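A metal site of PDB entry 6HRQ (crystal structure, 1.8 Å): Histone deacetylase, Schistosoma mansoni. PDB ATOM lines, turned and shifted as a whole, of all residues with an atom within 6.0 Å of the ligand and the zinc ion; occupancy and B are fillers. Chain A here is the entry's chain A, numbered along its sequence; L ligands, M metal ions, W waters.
Merely in contact with the ligand: Lys 21 (3.2 Å), Gly 151 (3.8 Å), Phe 152 (3.3 Å), Phe 217 (3.6 Å), Pro 292 (3.6 Å), His 293 (3.8 Å) and Gly 340 (3.9 Å). 13 residues have an atom within 4 Å of the ligand: Lys 21, His 142, His 143, Gly 151, Phe 152, Asp 187, His 189, Phe 217, Asp 286, Pro 292, His 293, Gly 340 and Tyr 342. The nearest printed residue that does not touch the ligand is Asp 101 (4.8 Å).
OD1 of Asp 286 is in hydrogen-bond range of N of Leu 188 (3.0 Å). OD2 of Asp 187 is in hydrogen-bond range of N of Gly 340 (3.1 Å). OD2 of Asp 187 sits at hydrogen-bond distance from NE2 of Gln 282 (3.1 Å). OD2 of Asp 291 lies within hydrogen-bond range of N of Tyr 342, at 2.9 Å. A ring nitrogen (NE2) of His 142 sits at hydrogen-bond distance from a ring nitrogen (NE2) of His 143, 3.3 Å away. The backbone NH (N) of His 143 sits at hydrogen-bond distance from the side-chain sulfur (SG) of Cys 153, at 3.6 Å. ND1 of His 293 sits at hydrogen-bond distance from OD1 of Asp 291 (2.7 Å). The backbone carbonyl oxygen (O) of Gly 151 sits at hydrogen-bond distance from the side-chain sulfur (SG) of Cys 153 (3.7 Å).
OH of Tyr 342 sits close to O2 of the ligand (2.5 Å). A nitrogen (N4) of the ligand lies within hydrogen-bond range of a ring nitrogen (NE2) of His 143 (2.8 Å). O1 of the ligand lies close to NE2 of His 142 (2.8 Å).
Three residues have an atom within 4 Å of the zinc ion: Asp 187, His 189 and Asp 286.
The zinc ion is bound by OD2 of Asp 286 (2.0 Å), OD1 of Asp 187 (2.1 Å), ND1 of His 189 (2.2 Å), O1 of the ligand (2.3 Å) and O2 of the ligand (2.3 Å).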
ATOM      1  N   LYS A  21      15.297 -21.801   5.239  1.00  0.00           N
ATOM      2  CA  LYS A  21      14.113 -21.358   4.516  1.00  0.00           C
ATOM      3  C   LYS A  21      14.464 -20.523   3.279  1.00  0.00           C
ATOM      4  O   LYS A  21      13.811 -20.645   2.235  1.00  0.00           O
ATOM      5  CB  LYS A  21      13.203 -20.547   5.426  1.00  0.00           C
ATOM      6  CG  LYS A  21      11.924 -20.121   4.762  1.00  0.00           C
ATOM      7  CD  LYS A  21      11.184 -21.342   4.247  1.00  0.00           C
ATOM      8  CE  LYS A  21      10.094 -20.985   3.249  1.00  0.00           C
ATOM      9  NZ  LYS A  21       9.353 -22.204   2.834  1.00  0.00           N
ATOM     10  N   PHE A  22      15.468 -19.646   3.382  1.00  0.00           N
ATOM     11  CA  PHE A  22      15.755 -18.727   2.285  1.00  0.00           C
ATOM     12  C   PHE A  22      16.994 -19.100   1.491  1.00  0.00           C
ATOM     13  O   PHE A  22      17.258 -18.472   0.455  1.00  0.00           O
ATOM     14  CB  PHE A  22      15.851 -17.290   2.831  1.00  0.00           C
ATOM     15  CG  PHE A  22      14.513 -16.730   3.249  1.00  0.00           C
ATOM     16  CD1 PHE A  22      13.599 -16.286   2.303  1.00  0.00           C
ATOM     17  CD2 PHE A  22      14.159 -16.681   4.593  1.00  0.00           C
ATOM     18  CE1 PHE A  22      12.353 -15.796   2.688  1.00  0.00           C
ATOM     19  CE2 PHE A  22      12.924 -16.186   4.997  1.00  0.00           C
ATOM     20  CZ  PHE A  22      12.018 -15.739   4.039  1.00  0.00           C
ATOM     21  N   ASP A 101       7.677 -22.893  12.357  1.00  0.00           N
ATOM     22  CA  ASP A 101       8.267 -22.149  11.256  1.00  0.00           C
ATOM     23  C   ASP A 101       9.468 -21.321  11.667  1.00  0.00           C
ATOM     24  O   ASP A 101      10.111 -20.722  10.792  1.00  0.00           O
ATOM     25  CB  ASP A 101       7.212 -21.246  10.604  1.00  0.00           C
ATOM     26  CG  ASP A 101       6.209 -22.022   9.801  1.00  0.00           C
ATOM     27  OD1 ASP A 101       6.591 -23.070   9.241  1.00  0.00           O
ATOM     28  OD2 ASP A 101       5.040 -21.597   9.741  1.00  0.00           O
ATOM     29  N   HIS A 142       9.318  -8.438   9.007  1.00  0.00           N
ATOM     30  CA  HIS A 142       8.323  -7.616   9.682  1.00  0.00           C
ATOM     31  C   HIS A 142       7.468  -8.345  10.714  1.00  0.00           C
ATOM     32  O   HIS A 142       6.699  -7.686  11.421  1.00  0.00           O
ATOM     33  CB  HIS A 142       7.386  -6.934   8.642  1.00  0.00           C
ATOM     34  CG  HIS A 142       6.727  -7.872   7.680  1.00  0.00           C
ATOM     35  ND1 HIS A 142       5.758  -7.439   6.788  1.00  0.00           N
ATOM     36  CD2 HIS A 142       6.893  -9.199   7.447  1.00  0.00           C
ATOM     37  CE1 HIS A 142       5.360  -8.466   6.051  1.00  0.00           C
ATOM     38  NE2 HIS A 142       6.031  -9.540   6.434  1.00  0.00           N
ATOM     39  N   HIS A 143       7.591  -9.680  10.857  1.00  0.00           N
ATOM     40  CA  HIS A 143       6.675 -10.406  11.743  1.00  0.00           C
ATOM     41  C   HIS A 143       7.172 -10.591  13.171  1.00  0.00           C
ATOM     42  O   HIS A 143       6.369 -10.943  14.044  1.00  0.00           O
ATOM     43  CB  HIS A 143       6.369 -11.813  11.182  1.00  0.00           C
ATOM     44  CG  HIS A 143       5.577 -11.815   9.921  1.00  0.00           C
ATOM     45  ND1 HIS A 143       4.381 -11.144   9.778  1.00  0.00           N
ATOM     46  CD2 HIS A 143       5.783 -12.455   8.738  1.00  0.00           C
ATOM     47  CE1 HIS A 143       3.899 -11.349   8.564  1.00  0.00           C
ATOM     48  NE2 HIS A 143       4.736 -12.130   7.910  1.00  0.00           N
ATOM     49  N   GLY A 151       6.666 -16.383  11.664  1.00  0.00           N
ATOM     50  CA  GLY A 151       6.703 -16.308  10.198  1.00  0.00           C
ATOM     51  C   GLY A 151       8.084 -16.225   9.575  1.00  0.00           C
ATOM     52  O   GLY A 151       8.297 -15.452   8.634  1.00  0.00           O
ATOM     53  N   PHE A 152       9.028 -17.038  10.070  1.00  0.00           N
ATOM     54  CA  PHE A 152      10.445 -17.065   9.652  1.00  0.00           C
ATOM     55  C   PHE A 152      11.220 -15.820  10.083  1.00  0.00           C
ATOM     56  O   PHE A 152      12.362 -15.638   9.644  1.00  0.00           O
ATOM     57  CB  PHE A 152      10.648 -17.214   8.136  1.00  0.00           C
ATOM     58  CG  PHE A 152       9.777 -18.267   7.480  1.00  0.00           C
ATOM     59  CD1 PHE A 152       9.481 -19.464   8.112  1.00  0.00           C
ATOM     60  CD2 PHE A 152       9.247 -18.038   6.213  1.00  0.00           C
ATOM     61  CE1 PHE A 152       8.669 -20.414   7.495  1.00  0.00           C
ATOM     62  CE2 PHE A 152       8.448 -18.993   5.595  1.00  0.00           C
ATOM     63  CZ  PHE A 152       8.158 -20.176   6.236  1.00  0.00           C
ATOM     64  N   CYS A 153      10.641 -14.957  10.922  1.00  0.00           N
ATOM     65  CA  CYS A 153      11.298 -13.750  11.415  1.00  0.00           C
ATOM     66  C   CYS A 153      11.658 -13.938  12.885  1.00  0.00           C
ATOM     67  O   CYS A 153      10.794 -14.263  13.701  1.00  0.00           O
ATOM     68  CB  CYS A 153      10.399 -12.517  11.272  1.00  0.00           C
ATOM     69  SG  CYS A 153       9.776 -12.230   9.587  1.00  0.00           S
ATOM     70  N   ASP A 187       4.386  -6.293   1.191  1.00  0.00           N
ATOM     71  CA  ASP A 187       4.422  -7.755   1.249  1.00  0.00           C
ATOM     72  C   ASP A 187       3.012  -8.361   1.082  1.00  0.00           C
ATOM     73  O   ASP A 187       2.008  -7.736   1.409  1.00  0.00           O
ATOM     74  CB  ASP A 187       5.015  -8.162   2.592  1.00  0.00           C
ATOM     75  CG  ASP A 187       5.483  -9.614   2.644  1.00  0.00           C
ATOM     76  OD1 ASP A 187       4.634 -10.514   2.871  1.00  0.00           O
ATOM     77  OD2 ASP A 187       6.695  -9.850   2.537  1.00  0.00           O
ATOM     78  N   LEU A 188       2.951  -9.607   0.582  1.00  0.00           N
ATOM     79  CA  LEU A 188       1.682 -10.334   0.542  1.00  0.00           C
ATOM     80  C   LEU A 188       1.021 -10.427   1.920  1.00  0.00           C
ATOM     81  O   LEU A 188      -0.216 -10.420   2.013  1.00  0.00           O
ATOM     82  CB  LEU A 188       1.885 -11.752   0.000  1.00  0.00           C
ATOM     83  CG  LEU A 188       0.627 -12.630  -0.132  1.00  0.00           C
ATOM     84  CD1 LEU A 188      -0.278 -12.066  -1.228  1.00  0.00           C
ATOM     85  CD2 LEU A 188       1.011 -14.062  -0.467  1.00  0.00           C
ATOM     86  N   HIS A 189       1.802 -10.500   2.986  1.00  0.00           N
ATOM     87  CA  HIS A 189       1.296 -10.681   4.336  1.00  0.00           C
ATOM     88  C   HIS A 189       1.186  -9.348   5.097  1.00  0.00           C
ATOM     89  O   HIS A 189       1.918  -8.390   4.825  1.00  0.00           O
ATOM     90  CB  HIS A 189       2.195 -11.646   5.126  1.00  0.00           C
ATOM     91  CG  HIS A 189       2.310 -13.005   4.507  1.00  0.00           C
ATOM     92  ND1 HIS A 189       3.302 -13.335   3.620  1.00  0.00           N
ATOM     93  CD2 HIS A 189       1.520 -14.101   4.621  1.00  0.00           C
ATOM     94  CE1 HIS A 189       3.135 -14.591   3.220  1.00  0.00           C
ATOM     95  NE2 HIS A 189       2.068 -15.085   3.822  1.00  0.00           N
ATOM     96  N   HIS A 190       0.258  -9.305   6.056  1.00  0.00           N
ATOM     97  CA  HIS A 190       0.132  -8.160   6.940  1.00  0.00           C
ATOM     98  C   HIS A 190       1.405  -7.965   7.757  1.00  0.00           C
ATOM     99  O   HIS A 190       1.926  -8.912   8.356  1.00  0.00           O
ATOM    100  CB  HIS A 190      -1.074  -8.345   7.877  1.00  0.00           C
ATOM    101  CG  HIS A 190      -1.205  -7.274   8.927  1.00  0.00           C
ATOM    102  ND1 HIS A 190      -1.313  -7.546  10.270  1.00  0.00           N
ATOM    103  CD2 HIS A 190      -1.275  -5.926   8.809  1.00  0.00           C
ATOM    104  CE1 HIS A 190      -1.434  -6.416  10.944  1.00  0.00           C
ATOM    105  NE2 HIS A 190      -1.430  -5.415  10.076  1.00  0.00           N
ATOM    106  N   PHE A 217      -2.250 -16.609   7.132  1.00  0.00           N
ATOM    107  CA  PHE A 217      -1.254 -15.998   8.017  1.00  0.00           C
ATOM    108  C   PHE A 217      -1.100 -14.492   7.779  1.00  0.00           C
ATOM    109  O   PHE A 217      -1.079 -14.068   6.625  1.00  0.00           O
ATOM    110  CB  PHE A 217       0.101 -16.698   7.817  1.00  0.00           C
ATOM    111  CG  PHE A 217       1.167 -16.282   8.798  1.00  0.00           C
ATOM    112  CD1 PHE A 217       1.326 -16.965   9.993  1.00  0.00           C
ATOM    113  CD2 PHE A 217       2.018 -15.219   8.520  1.00  0.00           C
ATOM    114  CE1 PHE A 217       2.298 -16.602  10.905  1.00  0.00           C
ATOM    115  CE2 PHE A 217       2.996 -14.843   9.430  1.00  0.00           C
ATOM    116  CZ  PHE A 217       3.141 -15.522  10.617  1.00  0.00           C
ATOM    117  N   GLN A 282       8.862  -1.782   2.900  1.00  0.00           N
ATOM    118  CA  GLN A 282       9.085  -3.222   2.850  1.00  0.00           C
ATOM    119  C   GLN A 282       8.560  -3.721   1.507  1.00  0.00           C
ATOM    120  O   GLN A 282       7.401  -3.474   1.156  1.00  0.00           O
ATOM    121  CB  GLN A 282       8.387  -3.923   4.028  1.00  0.00           C
ATOM    122  CG  GLN A 282       8.910  -5.321   4.393  1.00  0.00           C
ATOM    123  CD  GLN A 282       8.173  -6.428   3.649  1.00  0.00           C
ATOM    124  OE1 GLN A 282       7.541  -6.181   2.620  1.00  0.00           O
ATOM    125  NE2 GLN A 282       8.260  -7.660   4.161  1.00  0.00           N
ATOM    126  N   ASP A 286       6.383 -11.706  -2.499  1.00  0.00           N
ATOM    127  CA  ASP A 286       5.459 -12.820  -2.584  1.00  0.00           C
ATOM    128  C   ASP A 286       4.093 -12.450  -3.166  1.00  0.00           C
ATOM    129  O   ASP A 286       3.221 -13.325  -3.250  1.00  0.00           O
ATOM    130  CB  ASP A 286       5.298 -13.526  -1.209  1.00  0.00           C
ATOM    131  CG  ASP A 286       5.307 -12.566  -0.013  1.00  0.00           C
ATOM    132  OD1 ASP A 286       5.278 -11.332  -0.188  1.00  0.00           O
ATOM    133  OD2 ASP A 286       5.314 -13.087   1.125  1.00  0.00           O
ATOM    134  N   ASP A 291       4.983 -16.377  -7.631  1.00  0.00           N
ATOM    135  CA  ASP A 291       5.306 -16.899  -6.298  1.00  0.00           C
ATOM    136  C   ASP A 291       4.495 -18.163  -6.041  1.00  0.00           C
ATOM    137  O   ASP A 291       3.337 -18.244  -6.462  1.00  0.00           O
ATOM    138  CB  ASP A 291       5.023 -15.849  -5.224  1.00  0.00           C
ATOM    139  CG  ASP A 291       5.615 -16.224  -3.863  1.00  0.00           C
ATOM    140  OD1 ASP A 291       4.943 -16.969  -3.117  1.00  0.00           O
ATOM    141  OD2 ASP A 291       6.743 -15.789  -3.541  1.00  0.00           O
ATOM    142  N   PRO A 292       5.062 -19.176  -5.382  1.00  0.00           N
ATOM    143  CA  PRO A 292       4.289 -20.401  -5.120  1.00  0.00           C
ATOM    144  C   PRO A 292       3.018 -20.182  -4.314  1.00  0.00           C
ATOM    145  O   PRO A 292       2.124 -21.043  -4.347  1.00  0.00           O
ATOM    146  CB  PRO A 292       5.270 -21.311  -4.361  1.00  0.00           C
ATOM    147  CG  PRO A 292       6.592 -20.628  -4.404  1.00  0.00           C
ATOM    148  CD  PRO A 292       6.431 -19.230  -4.849  1.00  0.00           C
ATOM    149  N   HIS A 293       2.902 -19.070  -3.570  1.00  0.00           N
ATOM    150  CA  HIS A 293       1.625 -18.728  -2.942  1.00  0.00           C
ATOM    151  C   HIS A 293       0.506 -18.646  -3.970  1.00  0.00           C
ATOM    152  O   HIS A 293      -0.633 -19.059  -3.708  1.00  0.00           O
ATOM    153  CB  HIS A 293       1.726 -17.403  -2.178  1.00  0.00           C
ATOM    154  CG  HIS A 293       2.421 -17.517  -0.862  1.00  0.00           C
ATOM    155  ND1 HIS A 293       3.768 -17.254  -0.699  1.00  0.00           N
ATOM    156  CD2 HIS A 293       1.950 -17.837   0.374  1.00  0.00           C
ATOM    157  CE1 HIS A 293       4.092 -17.407   0.571  1.00  0.00           C
ATOM    158  NE2 HIS A 293       3.017 -17.761   1.245  1.00  0.00           N
ATOM    159  N   ARG A 294       0.800 -18.073  -5.146  1.00  0.00           N
ATOM    160  CA  ARG A 294      -0.191 -17.915  -6.209  1.00  0.00           C
ATOM    161  C   ARG A 294      -1.475 -17.274  -5.680  1.00  0.00           C
ATOM    162  O   ARG A 294      -2.576 -17.793  -5.877  1.00  0.00           O
ATOM    163  CB  ARG A 294      -0.479 -19.263  -6.865  1.00  0.00           C
ATOM    164  CG  ARG A 294       0.749 -19.982  -7.405  1.00  0.00           C
ATOM    165  CD  ARG A 294       1.283 -19.299  -8.659  1.00  0.00           C
ATOM    166  NE  ARG A 294       2.297 -20.091  -9.337  1.00  0.00           N
ATOM    167  CZ  ARG A 294       2.637 -19.937 -10.622  1.00  0.00           C
ATOM    168  NH1 ARG A 294       2.035 -19.018 -11.363  1.00  0.00           N
ATOM    169  NH2 ARG A 294       3.574 -20.715 -11.154  1.00  0.00           N
ATOM    170  N   GLY A 339      12.120  -8.819   2.132  1.00  0.00           N
ATOM    171  CA  GLY A 339      11.072  -9.508   2.855  1.00  0.00           C
ATOM    172  C   GLY A 339      10.756 -10.855   2.241  1.00  0.00           C
ATOM    173  O   GLY A 339      11.663 -11.599   1.860  1.00  0.00           O
ATOM    174  N   GLY A 340       9.475 -11.187   2.117  1.00  0.00           N
ATOM    175  CA  GLY A 340       9.080 -12.449   1.505  1.00  0.00           C
ATOM    176  C   GLY A 340       9.470 -12.540   0.030  1.00  0.00           C
ATOM    177  O   GLY A 340       9.915 -11.595  -0.618  1.00  0.00           O
ATOM    178  N   GLY A 341       9.291 -13.750  -0.503  1.00  0.00           N
ATOM    179  CA  GLY A 341       9.593 -14.050  -1.896  1.00  0.00           C
ATOM    180  C   GLY A 341      10.200 -15.437  -2.012  1.00  0.00           C
ATOM    181  O   GLY A 341      11.388 -15.640  -1.716  1.00  0.00           O
ATOM    182  N   TYR A 342       9.409 -16.417  -2.458  1.00  0.00           N
ATOM    183  CA  TYR A 342       9.806 -17.822  -2.383  1.00  0.00           C
ATOM    184  C   TYR A 342      10.058 -18.437  -3.753  1.00  0.00           C
ATOM    185  O   TYR A 342      10.397 -19.621  -3.838  1.00  0.00           O
ATOM    186  CB  TYR A 342       8.752 -18.576  -1.565  1.00  0.00           C
ATOM    187  CG  TYR A 342       8.630 -17.843  -0.243  1.00  0.00           C
ATOM    188  CD1 TYR A 342       9.564 -18.059   0.769  1.00  0.00           C
ATOM    189  CD2 TYR A 342       7.671 -16.844  -0.054  1.00  0.00           C
ATOM    190  CE1 TYR A 342       9.513 -17.341   1.975  1.00  0.00           C
ATOM    191  CE2 TYR A 342       7.625 -16.113   1.151  1.00  0.00           C
ATOM    192  CZ  TYR A 342       8.554 -16.375   2.145  1.00  0.00           C
ATOM    193  OH  TYR A 342       8.510 -15.677   3.342  1.00  0.00           O
HETATM  194  C1  LIG L   1       3.615 -21.196  -0.501  1.00  0.00           C
HETATM  195  C2  LIG L   1       2.497 -21.912  -0.916  1.00  0.00           C
HETATM  196  C3  LIG L   1       2.655 -23.154  -1.485  1.00  0.00           C
HETATM  197  C4  LIG L   1       5.028 -22.994  -1.230  1.00  0.00           C
HETATM  198  C5  LIG L   1       5.386 -19.341   4.002  1.00  0.00           C
HETATM  199  C6  LIG L   1       5.071 -15.991   6.604  1.00  0.00           C
HETATM  200  C7  LIG L   1       5.611 -15.817   5.332  1.00  0.00           C
HETATM  201  C8  LIG L   1       5.729 -16.930   4.497  1.00  0.00           C
HETATM  202  C9  LIG L   1       5.290 -18.183   4.913  1.00  0.00           C
HETATM  203  C10 LIG L   1       4.749 -18.325   6.193  1.00  0.00           C
HETATM  204  C11 LIG L   1       4.652 -17.235   7.028  1.00  0.00           C
HETATM  205  C12 LIG L   1       5.971 -14.447   4.845  1.00  0.00           C
HETATM  206  C13 LIG L   1       4.881 -21.726  -0.664  1.00  0.00           C
HETATM  207  C14 LIG L   1       3.916 -23.697  -1.647  1.00  0.00           C
HETATM  208  N1  LIG L   1       5.921 -20.806   2.520  1.00  0.00           N
HETATM  209  N2  LIG L   1       4.793 -21.239   3.104  1.00  0.00           N
HETATM  210  N3  LIG L   1       4.459 -20.345   4.011  1.00  0.00           N
HETATM  211  C15 LIG L   1       6.316 -19.644   3.048  1.00  0.00           C
HETATM  212  N4  LIG L   1       5.641 -13.436   5.644  1.00  0.00           N
HETATM  213  O1  LIG L   1       5.833 -12.114   5.234  1.00  0.00           O
HETATM  214  O2  LIG L   1       6.505 -14.292   3.745  1.00  0.00           O
HETATM  215  S1  LIG L   1       6.305 -20.812  -0.166  1.00  0.00           S
HETATM  216  C16 LIG L   1       6.580 -21.553   1.466  1.00  0.00           C
HETATM  217 ZN    ZN M   1       5.236 -12.503   3.066  1.00  0.00          ZN
HETATM  218  O   HOH W   1       2.145 -20.517   5.240  1.00  0.00           O
HETATM  219  O   HOH W   2       8.910 -11.495   5.321  1.00  0.00           O
